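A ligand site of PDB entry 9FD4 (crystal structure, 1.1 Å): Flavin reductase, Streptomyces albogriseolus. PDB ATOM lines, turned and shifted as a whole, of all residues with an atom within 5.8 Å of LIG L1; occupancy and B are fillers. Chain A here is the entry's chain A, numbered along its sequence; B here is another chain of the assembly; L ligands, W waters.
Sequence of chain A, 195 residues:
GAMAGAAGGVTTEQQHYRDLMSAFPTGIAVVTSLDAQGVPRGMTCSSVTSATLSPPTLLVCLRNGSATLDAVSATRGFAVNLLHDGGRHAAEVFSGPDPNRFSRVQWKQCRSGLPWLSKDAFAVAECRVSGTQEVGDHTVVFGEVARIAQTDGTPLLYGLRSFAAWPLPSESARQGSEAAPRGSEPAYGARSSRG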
ATOM      1  N   GLN A  15       6.863   8.935  29.570  1.00  0.00           N
ATOM      2  CA  GLN A  15       7.990   8.934  30.479  1.00  0.00           C
ATOM      3  C   GLN A  15       8.365   7.522  30.930  1.00  0.00           C
ATOM      4  O   GLN A  15       9.554   7.207  31.022  1.00  0.00           O
ATOM      5  CB  GLN A  15       7.683   9.814  31.701  1.00  0.00           C
ATOM      6  CG  GLN A  15       8.877   9.928  32.663  1.00  0.00           C
ATOM      7  CD  GLN A  15      10.015  10.657  32.024  1.00  0.00           C
ATOM      8  OE1 GLN A  15       9.848  11.786  31.556  1.00  0.00           O
ATOM      9  NE2 GLN A  15      11.186  10.046  32.015  1.00  0.00           N
ATOM     10  N   TYR A  17       8.121   4.889  29.178  1.00  0.00           N
ATOM     11  CA  TYR A  17       8.811   4.346  28.043  1.00  0.00           C
ATOM     12  C   TYR A  17      10.233   4.907  27.924  1.00  0.00           C
ATOM     13  O   TYR A  17      11.167   4.167  27.634  1.00  0.00           O
ATOM     14  CB  TYR A  17       7.973   4.582  26.775  1.00  0.00           C
ATOM     15  CG  TYR A  17       8.691   4.195  25.504  1.00  0.00           C
ATOM     16  CD1 TYR A  17       8.729   2.875  25.084  1.00  0.00           C
ATOM     17  CD2 TYR A  17       9.338   5.138  24.732  1.00  0.00           C
ATOM     18  CE1 TYR A  17       9.396   2.501  23.940  1.00  0.00           C
ATOM     19  CE2 TYR A  17      10.001   4.792  23.585  1.00  0.00           C
ATOM     20  CZ  TYR A  17      10.017   3.466  23.194  1.00  0.00           C
ATOM     21  OH  TYR A  17      10.688   3.081  22.066  1.00  0.00           O
ATOM     22  N   ARG A  18      10.393   6.227  28.105  1.00  0.00           N
ATOM     23  CA  ARG A  18      11.720   6.808  28.146  1.00  0.00           C
ATOM     24  C   ARG A  18      12.583   6.142  29.201  1.00  0.00           C
ATOM     25  O   ARG A  18      13.769   5.857  28.957  1.00  0.00           O
ATOM     26  CB  ARG A  18      11.616   8.305  28.433  1.00  0.00           C
ATOM     27  CG  ARG A  18      11.081   9.125  27.281  1.00  0.00           C
ATOM     28  CD  ARG A  18      11.178  10.632  27.504  1.00  0.00           C
ATOM     29  NE  ARG A  18      11.504  11.301  26.252  1.00  0.00           N
ATOM     30  CZ  ARG A  18      11.795  12.581  26.121  1.00  0.00           C
ATOM     31  NH1 ARG A  18      11.768  13.405  27.167  1.00  0.00           N
ATOM     32  NH2 ARG A  18      12.116  13.063  24.923  1.00  0.00           N
ATOM     33  N   ASP A  19      12.018   5.871  30.384  1.00  0.00           N
ATOM     34  CA  ASP A  19      12.772   5.226  31.462  1.00  0.00           C
ATOM     35  C   ASP A  19      13.279   3.851  31.042  1.00  0.00           C
ATOM     36  O   ASP A  19      14.391   3.442  31.382  1.00  0.00           O
ATOM     37  CB  ASP A  19      11.918   5.125  32.730  1.00  0.00           C
ATOM     38  CG  ASP A  19      11.617   6.469  33.386  1.00  0.00           C
ATOM     39  OD1 ASP A  19      12.226   7.493  33.059  1.00  0.00           O
ATOM     40  OD2 ASP A  19      10.738   6.470  34.289  1.00  0.00           O
ATOM     41  N   MET A  21      13.796   2.780  27.768  1.00  0.00           N
ATOM     42  CA  MET A  21      14.799   2.855  26.719  1.00  0.00           C
ATOM     43  C   MET A  21      16.097   3.490  27.192  1.00  0.00           C
ATOM     44  O   MET A  21      17.161   3.165  26.660  1.00  0.00           O
ATOM     45  CB  MET A  21      14.205   3.562  25.511  1.00  0.00           C
ATOM     46  CG  MET A  21      12.952   2.863  24.913  1.00  0.00           C
ATOM     47  SD  MET A  21      13.045   1.104  24.598  1.00  0.00           S
ATOM     48  CE  MET A  21      14.179   1.146  23.280  1.00  0.00           C
ATOM     49  N   SER A  22      16.028   4.333  28.201  1.00  0.00           N
ATOM     50  CA  SER A  22      17.254   4.867  28.775  1.00  0.00           C
ATOM     51  C   SER A  22      18.153   3.731  29.238  1.00  0.00           C
ATOM     52  O   SER A  22      19.388   3.849  29.165  1.00  0.00           O
ATOM     53  CB  SER A  22      16.890   5.783  29.938  1.00  0.00           C
ATOM     54  OG  SER A  22      18.035   6.316  30.561  1.00  0.00           O
ATOM     55  N   SER A  46      21.381   7.508  18.312  1.00  0.00           N
ATOM     56  CA  SER A  46      21.616   6.250  18.984  1.00  0.00           C
ATOM     57  C   SER A  46      20.778   5.129  18.409  1.00  0.00           C
ATOM     58  O   SER A  46      20.901   4.009  18.871  1.00  0.00           O
ATOM     59  CB  SER A  46      21.334   6.361  20.484  1.00  0.00           C
ATOM     60  OG  SER A  46      20.009   6.830  20.753  1.00  0.00           O
ATOM     61  N   SER A  47      19.986   5.381  17.370  1.00  0.00           N
ATOM     62  CA  SER A  47      19.075   4.388  16.784  1.00  0.00           C
ATOM     63  C   SER A  47      19.702   3.539  15.656  1.00  0.00           C
ATOM     64  O   SER A  47      18.990   2.836  14.907  1.00  0.00           O
ATOM     65  CB  SER A  47      17.787   5.053  16.302  1.00  0.00           C
ATOM     66  OG  SER A  47      18.060   6.006  15.317  1.00  0.00           O
ATOM     67  N   CYS A  61      16.592   5.852  12.880  1.00  0.00           N
ATOM     68  CA  CYS A  61      15.253   6.401  13.071  1.00  0.00           C
ATOM     69  C   CYS A  61      15.358   7.873  13.446  1.00  0.00           C
ATOM     70  O   CYS A  61      15.848   8.202  14.533  1.00  0.00           O
ATOM     71  CB  CYS A  61      14.505   5.585  14.133  1.00  0.00           C
ATOM     72  SG  CYS A  61      12.773   5.978  14.157  1.00  0.00           S
ATOM     73  N   ARG A  63      13.760  12.001  13.486  1.00  0.00           N
ATOM     74  CA  ARG A  63      12.551  12.777  13.718  1.00  0.00           C
ATOM     75  C   ARG A  63      12.059  13.450  12.455  1.00  0.00           C
ATOM     76  O   ARG A  63      12.821  14.125  11.746  1.00  0.00           O
ATOM     77  CB  ARG A  63      12.846  13.846  14.749  1.00  0.00           C
ATOM     78  CG  ARG A  63      11.580  14.598  15.198  1.00  0.00           C
ATOM     79  CD  ARG A  63      11.893  15.815  16.052  1.00  0.00           C
ATOM     80  NE  ARG A  63      12.109  16.995  15.226  1.00  0.00           N
ATOM     81  CZ  ARG A  63      13.207  17.719  15.172  1.00  0.00           C
ATOM     82  NH1 ARG A  63      14.329  17.319  15.759  1.00  0.00           N
ATOM     83  NH2 ARG A  63      13.206  18.863  14.500  1.00  0.00           N
ATOM     84  N   ASP A 137       5.866  10.175  14.670  1.00  0.00           N
ATOM     85  CA  ASP A 137       6.500  11.405  14.207  1.00  0.00           C
ATOM     86  C   ASP A 137       7.960  11.201  13.840  1.00  0.00           C
ATOM     87  O   ASP A 137       8.732  12.172  13.822  1.00  0.00           O
ATOM     88  CB  ASP A 137       6.355  12.523  15.225  1.00  0.00           C
ATOM     89  CG  ASP A 137       6.824  12.128  16.587  1.00  0.00           C
ATOM     90  OD1 ASP A 137       7.505  11.091  16.701  1.00  0.00           O
ATOM     91  OD2 ASP A 137       6.502  12.852  17.543  1.00  0.00           O
ATOM     92  N   HIS A 138       8.338   9.963  13.560  1.00  0.00           N
ATOM     93  CA  HIS A 138       9.685   9.637  13.123  1.00  0.00           C
ATOM     94  C   HIS A 138       9.626   8.862  11.831  1.00  0.00           C
ATOM     95  O   HIS A 138       8.557   8.401  11.406  1.00  0.00           O
ATOM     96  CB  HIS A 138      10.388   8.845  14.208  1.00  0.00           C
ATOM     97  CG  HIS A 138      10.716   9.696  15.401  1.00  0.00           C
ATOM     98  ND1 HIS A 138       9.732  10.214  16.220  1.00  0.00           N
ATOM     99  CD2 HIS A 138      11.877  10.234  15.842  1.00  0.00           C
ATOM    100  CE1 HIS A 138      10.276  10.976  17.140  1.00  0.00           C
ATOM    101  NE2 HIS A 138      11.579  10.989  16.943  1.00  0.00           N
ATOM    102  N   TYR A 158      26.297   5.866  25.376  1.00  0.00           N
ATOM    103  CA  TYR A 158      25.315   6.658  26.105  1.00  0.00           C
ATOM    104  C   TYR A 158      24.291   5.709  26.687  1.00  0.00           C
ATOM    105  O   TYR A 158      23.800   4.819  25.990  1.00  0.00           O
ATOM    106  CB  TYR A 158      24.624   7.673  25.207  1.00  0.00           C
ATOM    107  CG  TYR A 158      23.851   8.704  25.962  1.00  0.00           C
ATOM    108  CD1 TYR A 158      24.462   9.857  26.461  1.00  0.00           C
ATOM    109  CD2 TYR A 158      22.499   8.560  26.178  1.00  0.00           C
ATOM    110  CE1 TYR A 158      23.762  10.800  27.155  1.00  0.00           C
ATOM    111  CE2 TYR A 158      21.767   9.507  26.872  1.00  0.00           C
ATOM    112  CZ  TYR A 158      22.406  10.645  27.352  1.00  0.00           C
ATOM    113  OH  TYR A 158      21.713  11.603  28.041  1.00  0.00           O
ATOM    114  N   ARG A 161      21.104   8.001  30.985  1.00  0.00           N
ATOM    115  CA  ARG A 161      21.189   9.437  30.980  1.00  0.00           C
ATOM    116  C   ARG A 161      22.610   9.956  31.215  1.00  0.00           C
ATOM    117  O   ARG A 161      22.809  11.018  31.820  1.00  0.00           O
ATOM    118  CB  ARG A 161      20.149  10.008  31.958  1.00  0.00           C
ATOM    119  CG  ARG A 161      18.747   9.341  31.721  1.00  0.00           C
ATOM    120  CD  ARG A 161      17.624  10.110  32.295  1.00  0.00           C
ATOM    121  NE  ARG A 161      16.366   9.600  31.762  1.00  0.00           N
ATOM    122  CZ  ARG A 161      15.566   8.768  32.404  1.00  0.00           C
ATOM    123  NH1 ARG A 161      15.836   8.347  33.626  1.00  0.00           N
ATOM    124  NH2 ARG A 161      14.459   8.363  31.802  1.00  0.00           N
ATOM    125  N   SER A 162      23.607   9.215  30.725  1.00  0.00           N
ATOM    126  CA  SER A 162      25.009   9.577  30.887  1.00  0.00           C
ATOM    127  C   SER A 162      25.827   9.091  29.705  1.00  0.00           C
ATOM    128  O   SER A 162      25.526   8.056  29.112  1.00  0.00           O
ATOM    129  CB  SER A 162      25.592   8.942  32.152  1.00  0.00           C
ATOM    130  OG  SER A 162      26.925   9.345  32.339  1.00  0.00           O
ATOM    131  N   SER B  50      14.495   2.349  19.685  1.00  0.00           N
ATOM    132  CA  SER B  50      13.336   3.204  19.885  1.00  0.00           C
ATOM    133  C   SER B  50      12.917   3.819  18.570  1.00  0.00           C
ATOM    134  O   SER B  50      13.750   4.300  17.810  1.00  0.00           O
ATOM    135  CB  SER B  50      13.693   4.281  20.878  1.00  0.00           C
ATOM    136  OG  SER B  50      12.510   4.932  21.265  1.00  0.00           O
ATOM    137  N   ALA B  51      11.622   3.863  18.320  1.00  0.00           N
ATOM    138  CA  ALA B  51      11.127   4.494  17.117  1.00  0.00           C
ATOM    139  C   ALA B  51      10.405   5.809  17.363  1.00  0.00           C
ATOM    140  O   ALA B  51      10.768   6.818  16.751  1.00  0.00           O
ATOM    141  CB  ALA B  51      10.265   3.533  16.321  1.00  0.00           C
ATOM    142  N   THR B  52       9.374   5.814  18.198  1.00  0.00           N
ATOM    143  CA  THR B  52       8.638   7.041  18.448  1.00  0.00           C
ATOM    144  C   THR B  52       7.995   6.985  19.827  1.00  0.00           C
ATOM    145  O   THR B  52       7.815   5.903  20.407  1.00  0.00           O
ATOM    146  CB  THR B  52       7.609   7.302  17.331  1.00  0.00           C
ATOM    147  OG1 THR B  52       7.090   8.617  17.440  1.00  0.00           O
ATOM    148  CG2 THR B  52       6.468   6.294  17.392  1.00  0.00           C
ATOM    149  N   LEU B  53       7.591   8.151  20.317  1.00  0.00           N
ATOM    150  CA  LEU B  53       6.856   8.254  21.573  1.00  0.00           C
ATOM    151  C   LEU B  53       5.358   8.330  21.382  1.00  0.00           C
ATOM    152  O   LEU B  53       4.630   8.199  22.360  1.00  0.00           O
ATOM    153  CB  LEU B  53       7.252   9.488  22.390  1.00  0.00           C
ATOM    154  CG  LEU B  53       8.679   9.623  22.799  1.00  0.00           C
ATOM    155  CD1 LEU B  53       8.847  10.871  23.616  1.00  0.00           C
ATOM    156  CD2 LEU B  53       9.130   8.414  23.558  1.00  0.00           C
HETATM  157  P1  LIG L   1      15.239  10.513  28.186  1.00  0.00           P
HETATM  158  O1  LIG L   1      14.737  11.801  27.655  1.00  0.00           O
HETATM  159  O2  LIG L   1      14.576   9.986  29.451  1.00  0.00           O
HETATM  160  O3  LIG L   1      15.194   9.409  26.991  1.00  0.00           O
HETATM  161  C1  LIG L   1      15.413   8.038  27.237  1.00  0.00           C
HETATM  162  C2  LIG L   1      15.346   7.248  25.949  1.00  0.00           C
HETATM  163  O4  LIG L   1      14.012   7.336  25.384  1.00  0.00           O
HETATM  164  C3  LIG L   1      16.251   7.770  24.826  1.00  0.00           C
HETATM  165  O5  LIG L   1      17.555   7.293  25.006  1.00  0.00           O
HETATM  166  C4  LIG L   1      15.536   7.130  23.624  1.00  0.00           C
HETATM  167  O6  LIG L   1      15.795   5.768  23.416  1.00  0.00           O
HETATM  168  C5  LIG L   1      14.055   7.295  23.981  1.00  0.00           C
HETATM  169  N1  LIG L   1      13.428   8.500  23.464  1.00  0.00           N
HETATM  170  C6  LIG L   1      13.441   9.747  24.031  1.00  0.00           C
HETATM  171  N2  LIG L   1      12.811  10.641  23.346  1.00  0.00           N
HETATM  172  C7  LIG L   1      12.366   9.960  22.226  1.00  0.00           C
HETATM  173  C8  LIG L   1      11.609  10.349  21.112  1.00  0.00           C
HETATM  174  N3  LIG L   1      11.163  11.598  20.919  1.00  0.00           N
HETATM  175  N4  LIG L   1      11.318   9.407  20.213  1.00  0.00           N
HETATM  176  C9  LIG L   1      11.748   8.153  20.381  1.00  0.00           C
HETATM  177  N5  LIG L   1      12.454   7.672  21.390  1.00  0.00           N
HETATM  178  C10 LIG L   1      12.721   8.633  22.284  1.00  0.00           C
HETATM  179  N6  LIG L   1      14.756  14.699  20.860  1.00  0.00           N
HETATM  180  C11 LIG L   1      13.913  15.684  20.498  1.00  0.00           C
HETATM  181  O7  LIG L   1      13.986  16.811  20.946  1.00  0.00           O
HETATM  182  N7  LIG L   1      12.939  15.400  19.549  1.00  0.00           N
HETATM  183  C12 LIG L   1      12.716  14.197  18.936  1.00  0.00           C
HETATM  184  O8  LIG L   1      11.843  14.001  18.125  1.00  0.00           O
HETATM  185  C13 LIG L   1      13.668  13.152  19.348  1.00  0.00           C
HETATM  186  N8  LIG L   1      13.568  11.974  18.820  1.00  0.00           N
HETATM  187  C14 LIG L   1      14.407  10.986  19.205  1.00  0.00           C
HETATM  188  C15 LIG L   1      14.290   9.720  18.629  1.00  0.00           C
HETATM  189  C16 LIG L   1      15.099   8.664  18.960  1.00  0.00           C
HETATM  190  C17 LIG L   1      14.923   7.322  18.293  1.00  0.00           C
HETATM  191  C18 LIG L   1      16.081   8.892  19.968  1.00  0.00           C
HETATM  192  C19 LIG L   1      17.042   7.816  20.406  1.00  0.00           C
HETATM  193  C20 LIG L   1      16.205  10.140  20.568  1.00  0.00           C
HETATM  194  C21 LIG L   1      15.376  11.212  20.202  1.00  0.00           C
HETATM  195  N9  LIG L   1      15.488  12.505  20.723  1.00  0.00           N
HETATM  196  C22 LIG L   1      14.639  13.492  20.340  1.00  0.00           C
HETATM  197  C23 LIG L   1      16.470  12.792  21.788  1.00  0.00           C
HETATM  198  C24 LIG L   1      15.862  12.352  23.128  1.00  0.00           C
HETATM  199  O9  LIG L   1      14.706  13.096  23.398  1.00  0.00           O
HETATM  200  C25 LIG L   1      16.847  12.452  24.283  1.00  0.00           C
HETATM  201  O10 LIG L   1      17.238  13.791  24.486  1.00  0.00           O
HETATM  202  C26 LIG L   1      18.132  11.642  24.015  1.00  0.00           C
HETATM  203  O11 LIG L   1      17.799  10.393  23.451  1.00  0.00           O
HETATM  204  C27 LIG L   1      18.877  11.531  25.315  1.00  0.00           C
HETATM  205  O12 LIG L   1      17.845  11.299  26.294  1.00  0.00           O
HETATM  206  P2  LIG L   1      18.174  10.585  27.677  1.00  0.00           P
HETATM  207  O13 LIG L   1      18.402   9.134  27.322  1.00  0.00           O
HETATM  208  O14 LIG L   1      19.268  11.269  28.338  1.00  0.00           O
HETATM  209  O15 LIG L   1      16.810  10.627  28.550  1.00  0.00           O
HETATM  210  P1  LG2 L   2      16.615  20.140  14.160  1.00  0.00           P
HETATM  211  O1  LG2 L   2      15.934  20.432  12.874  1.00  0.00           O
HETATM  212  O2  LG2 L   2      15.848  19.872  15.406  1.00  0.00           O
HETATM  213  O3  LG2 L   2      17.596  21.366  14.425  1.00  0.00           O
HETATM  214  C1  LG2 L   2      18.429  21.520  15.562  1.00  0.00           C
HETATM  215  C2  LG2 L   2      18.426  22.992  15.956  1.00  0.00           C
HETATM  216  O4  LG2 L   2      18.766  23.804  14.794  1.00  0.00           O
HETATM  217  C3  LG2 L   2      17.103  23.560  16.464  1.00  0.00           C
HETATM  218  O5  LG2 L   2      17.371  24.648  17.351  1.00  0.00           O
HETATM  219  C4  LG2 L   2      16.493  24.046  15.136  1.00  0.00           C
HETATM  220  O6  LG2 L   2      15.531  25.028  15.333  1.00  0.00           O
HETATM  221  C5  LG2 L   2      17.703  24.608  14.375  1.00  0.00           C
HETATM  222  N1  LG2 L   2      17.652  24.572  12.927  1.00  0.00           N
HETATM  223  C6  LG2 L   2      17.401  23.495  12.108  1.00  0.00           C
HETATM  224  N2  LG2 L   2      17.469  23.762  10.838  1.00  0.00           N
HETATM  225  C7  LG2 L   2      17.788  25.100  10.793  1.00  0.00           C
HETATM  226  C8  LG2 L   2      18.002  26.007   9.727  1.00  0.00           C
HETATM  227  N3  LG2 L   2      17.920  25.648   8.444  1.00  0.00           N
HETATM  228  N4  LG2 L   2      18.308  27.273  10.029  1.00  0.00           N
HETATM  229  C9  LG2 L   2      18.402  27.628  11.317  1.00  0.00           C
HETATM  230  N5  LG2 L   2      18.221  26.875  12.387  1.00  0.00           N
HETATM  231  C10 LG2 L   2      17.912  25.615  12.077  1.00  0.00           C
HETATM  232  N6  LG2 L   2      17.092  12.148  17.429  1.00  0.00           N
HETATM  233  C11 LG2 L   2      16.550  11.352  16.470  1.00  0.00           C
HETATM  234  O7  LG2 L   2      15.663  11.742  15.704  1.00  0.00           O
HETATM  235  N7  LG2 L   2      17.017  10.031  16.398  1.00  0.00           N
HETATM  236  C12 LG2 L   2      17.951   9.461  17.183  1.00  0.00           C
HETATM  237  O8  LG2 L   2      18.319   8.307  17.047  1.00  0.00           O
HETATM  238  C13 LG2 L   2      18.488  10.325  18.221  1.00  0.00           C
HETATM  239  N8  LG2 L   2      19.402   9.851  19.032  1.00  0.00           N
HETATM  240  C14 LG2 L   2      19.930  10.688  19.987  1.00  0.00           C
HETATM  241  C15 LG2 L   2      20.904  10.194  20.869  1.00  0.00           C
HETATM  242  C16 LG2 L   2      21.484  10.968  21.852  1.00  0.00           C
HETATM  243  C17 LG2 L   2      22.505  10.369  22.769  1.00  0.00           C
HETATM  244  C18 LG2 L   2      21.084  12.314  21.949  1.00  0.00           C
HETATM  245  C19 LG2 L   2      21.682  13.214  22.994  1.00  0.00           C
HETATM  246  C20 LG2 L   2      20.158  12.811  21.055  1.00  0.00           C
HETATM  247  C21 LG2 L   2      19.543  12.039  20.058  1.00  0.00           C
HETATM  248  N9  LG2 L   2      18.609  12.491  19.159  1.00  0.00           N
HETATM  249  C22 LG2 L   2      18.023  11.681  18.228  1.00  0.00           C
HETATM  250  C23 LG2 L   2      18.159  13.911  19.160  1.00  0.00           C
HETATM  251  C24 LG2 L   2      18.916  14.692  18.043  1.00  0.00           C
HETATM  252  O9  LG2 L   2      20.315  14.493  18.095  1.00  0.00           O
HETATM  253  C25 LG2 L   2      18.644  16.197  18.157  1.00  0.00           C
HETATM  254  O10 LG2 L   2      17.234  16.364  18.135  1.00  0.00           O
HETATM  255  C26 LG2 L   2      19.323  17.047  17.076  1.00  0.00           C
HETATM  256  O11 LG2 L   2      19.429  18.381  17.540  1.00  0.00           O
HETATM  257  C27 LG2 L   2      18.612  17.000  15.752  1.00  0.00           C
HETATM  258  O12 LG2 L   2      19.370  17.820  14.856  1.00  0.00           O
HETATM  259  P2  LG2 L   2      18.848  18.316  13.431  1.00  0.00           P
HETATM  260  O13 LG2 L   2      19.709  19.454  13.025  1.00  0.00           O
HETATM  261  O14 LG2 L   2      18.586  17.195  12.519  1.00  0.00           O
HETATM  262  O15 LG2 L   2      17.403  18.838  13.852  1.00  0.00           O
HETATM  263  O   HOH W   1      11.705  14.083  22.587  1.00  0.00           O
HETATM  264  O   HOH W   2      18.762  15.858  22.216  1.00  0.00           O
HETATM  265  O   HOH W   3      19.653   7.378  28.667  1.00  0.00           O
HETATM  266  O   HOH W   4      19.801   8.022  23.269  1.00  0.00           O
HETATM  267  O   HOH W   5      18.260   5.109  22.001  1.00  0.00           O
HETATM  268  O   HOH W   6      13.439  11.656  30.894  1.00  0.00           O
HETATM  269  O   HOH W   7      16.767  17.211  20.727  1.00  0.00           O
HETATM  270  O   HOH W   8      11.198  17.603  19.041  1.00  0.00           O
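OG of Ser 50 of chain B sits at hydrogen-bond distance from OH of Tyr 17, 2.7 Å away. The guanidinium group (NH2) of Arg 161 lies within salt-bridge range of the side-chain carboxylate (OD1) of Asp 19, at 2.7 Å. ND1 of His 138 sits at hydrogen-bond distance from OG1 of Thr 52 of chain B (3.3 Å). The side-chain carboxylate (OD1) of Asp 137 sits at hydrogen-bond distance from a ring nitrogen (ND1) of His 138 (2.4 Å). OG1 of Thr 52 of chain B lies within hydrogen-bond range of OD1 of Asp 137 (2.6 Å). O of Ala 51 of chain B lies within hydrogen-bond range of SG of Cys 61 (3.4 Å). The backbone NH (N) of Cys 61 lies within hydrogen-bond range of the side-chain hydroxyl (OG) of Ser 47 (2.8 Å).
OH of Tyr 158 lies within hydrogen-bond range of O14 of LIG L1 (2.5 Å). OG of Ser 50 of chain B is in hydrogen-bond range of N5 of LIG L1 (2.7 Å). NH2 of Arg 161 lies within salt-bridge range of O2 of LIG L1. A ring nitrogen (NE2) of His 138 sits at hydrogen-bond distance from a nitrogen (N8) of LIG L1 (2.9 Å). An oxygen (O1) of LIG L1 is in salt-bridge range of the guanidinium group of Arg 18. O7 of LG2 L2 sits at hydrogen-bond distance from N of Arg 63, at 2.9 Å. The guanidinium group of Arg 63 lies within salt-bridge range of an oxygen (O2) of LG2 L2 (3.0 Å). The backbone NH (N) of Ser 46 lies within hydrogen-bond range of a nitrogen (N8) of LG2 L2 (3.2 Å). O of Cys 61 sits at hydrogen-bond distance from N7 of LG2 L2, at 2.9 Å. The backbone NH (N) of Ser 47 lies close to an oxygen (O8) of LG2 L2 (3.4 Å). OG of Ser 47 is in hydrogen-bond range of O8 of LG2 L2 (2.9 Å).
Water W6 bridges an oxygen (O2) of LIG L1 and the side-chain amide nitrogen (NE2) of Gln 15. Water W3 lies within hydrogen-bond range of O13 of LIG L1 (2.5 Å), OG of Ser 22 (2.7 Å) and N of Arg 161 (2.8 Å). Water W7 lies within hydrogen-bond range of O10 of LG2 L2 and O7 of LIG L1. Water W5 bridges OG of Ser 46 (2.8 Å) and O6 of LIG L1 (2.9 Å). Water W4 lies within hydrogen-bond range of OG of Ser 46 (2.8 Å) and O5 of LIG L1 (2.9 Å). Water W1 lies within hydrogen-bond range of the guanidinium group (NH2) of Arg 18 (2.6 Å) and a nitrogen (N3) of LIG L1 (3.0 Å).
CB of Met 21 touches O6 of LIG L1 (3.4 Å). Ser 22 touches LIG L1. OG of Ser 46 touches C19 of LIG L1, at 3.1 Å. Cys 61 touches LIG L1. Arg 63 touches LIG L1 (CD to O8, 2.8 Å). O of Ala 51 of chain B touches C9 of LIG L1, 3.99 Å away. CA of Thr 52 of chain B touches C9 of LIG L1 (3.8 Å). CG of Leu 53 of chain B touches C8 of LIG L1, at 3.5 Å. Within 4 Å of LIG L1: Arg 18, Met 21, Ser 22, Ser 46, Cys 61, Arg 63, His 138, Tyr 158, Arg 161, Ser 50 of chain B, Ala 51 of chain B, Thr 52 of chain B and Leu 53 of chain B. The nearest printed residue that does not touch LIG L1 is Ser 47 (4.2 Å).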
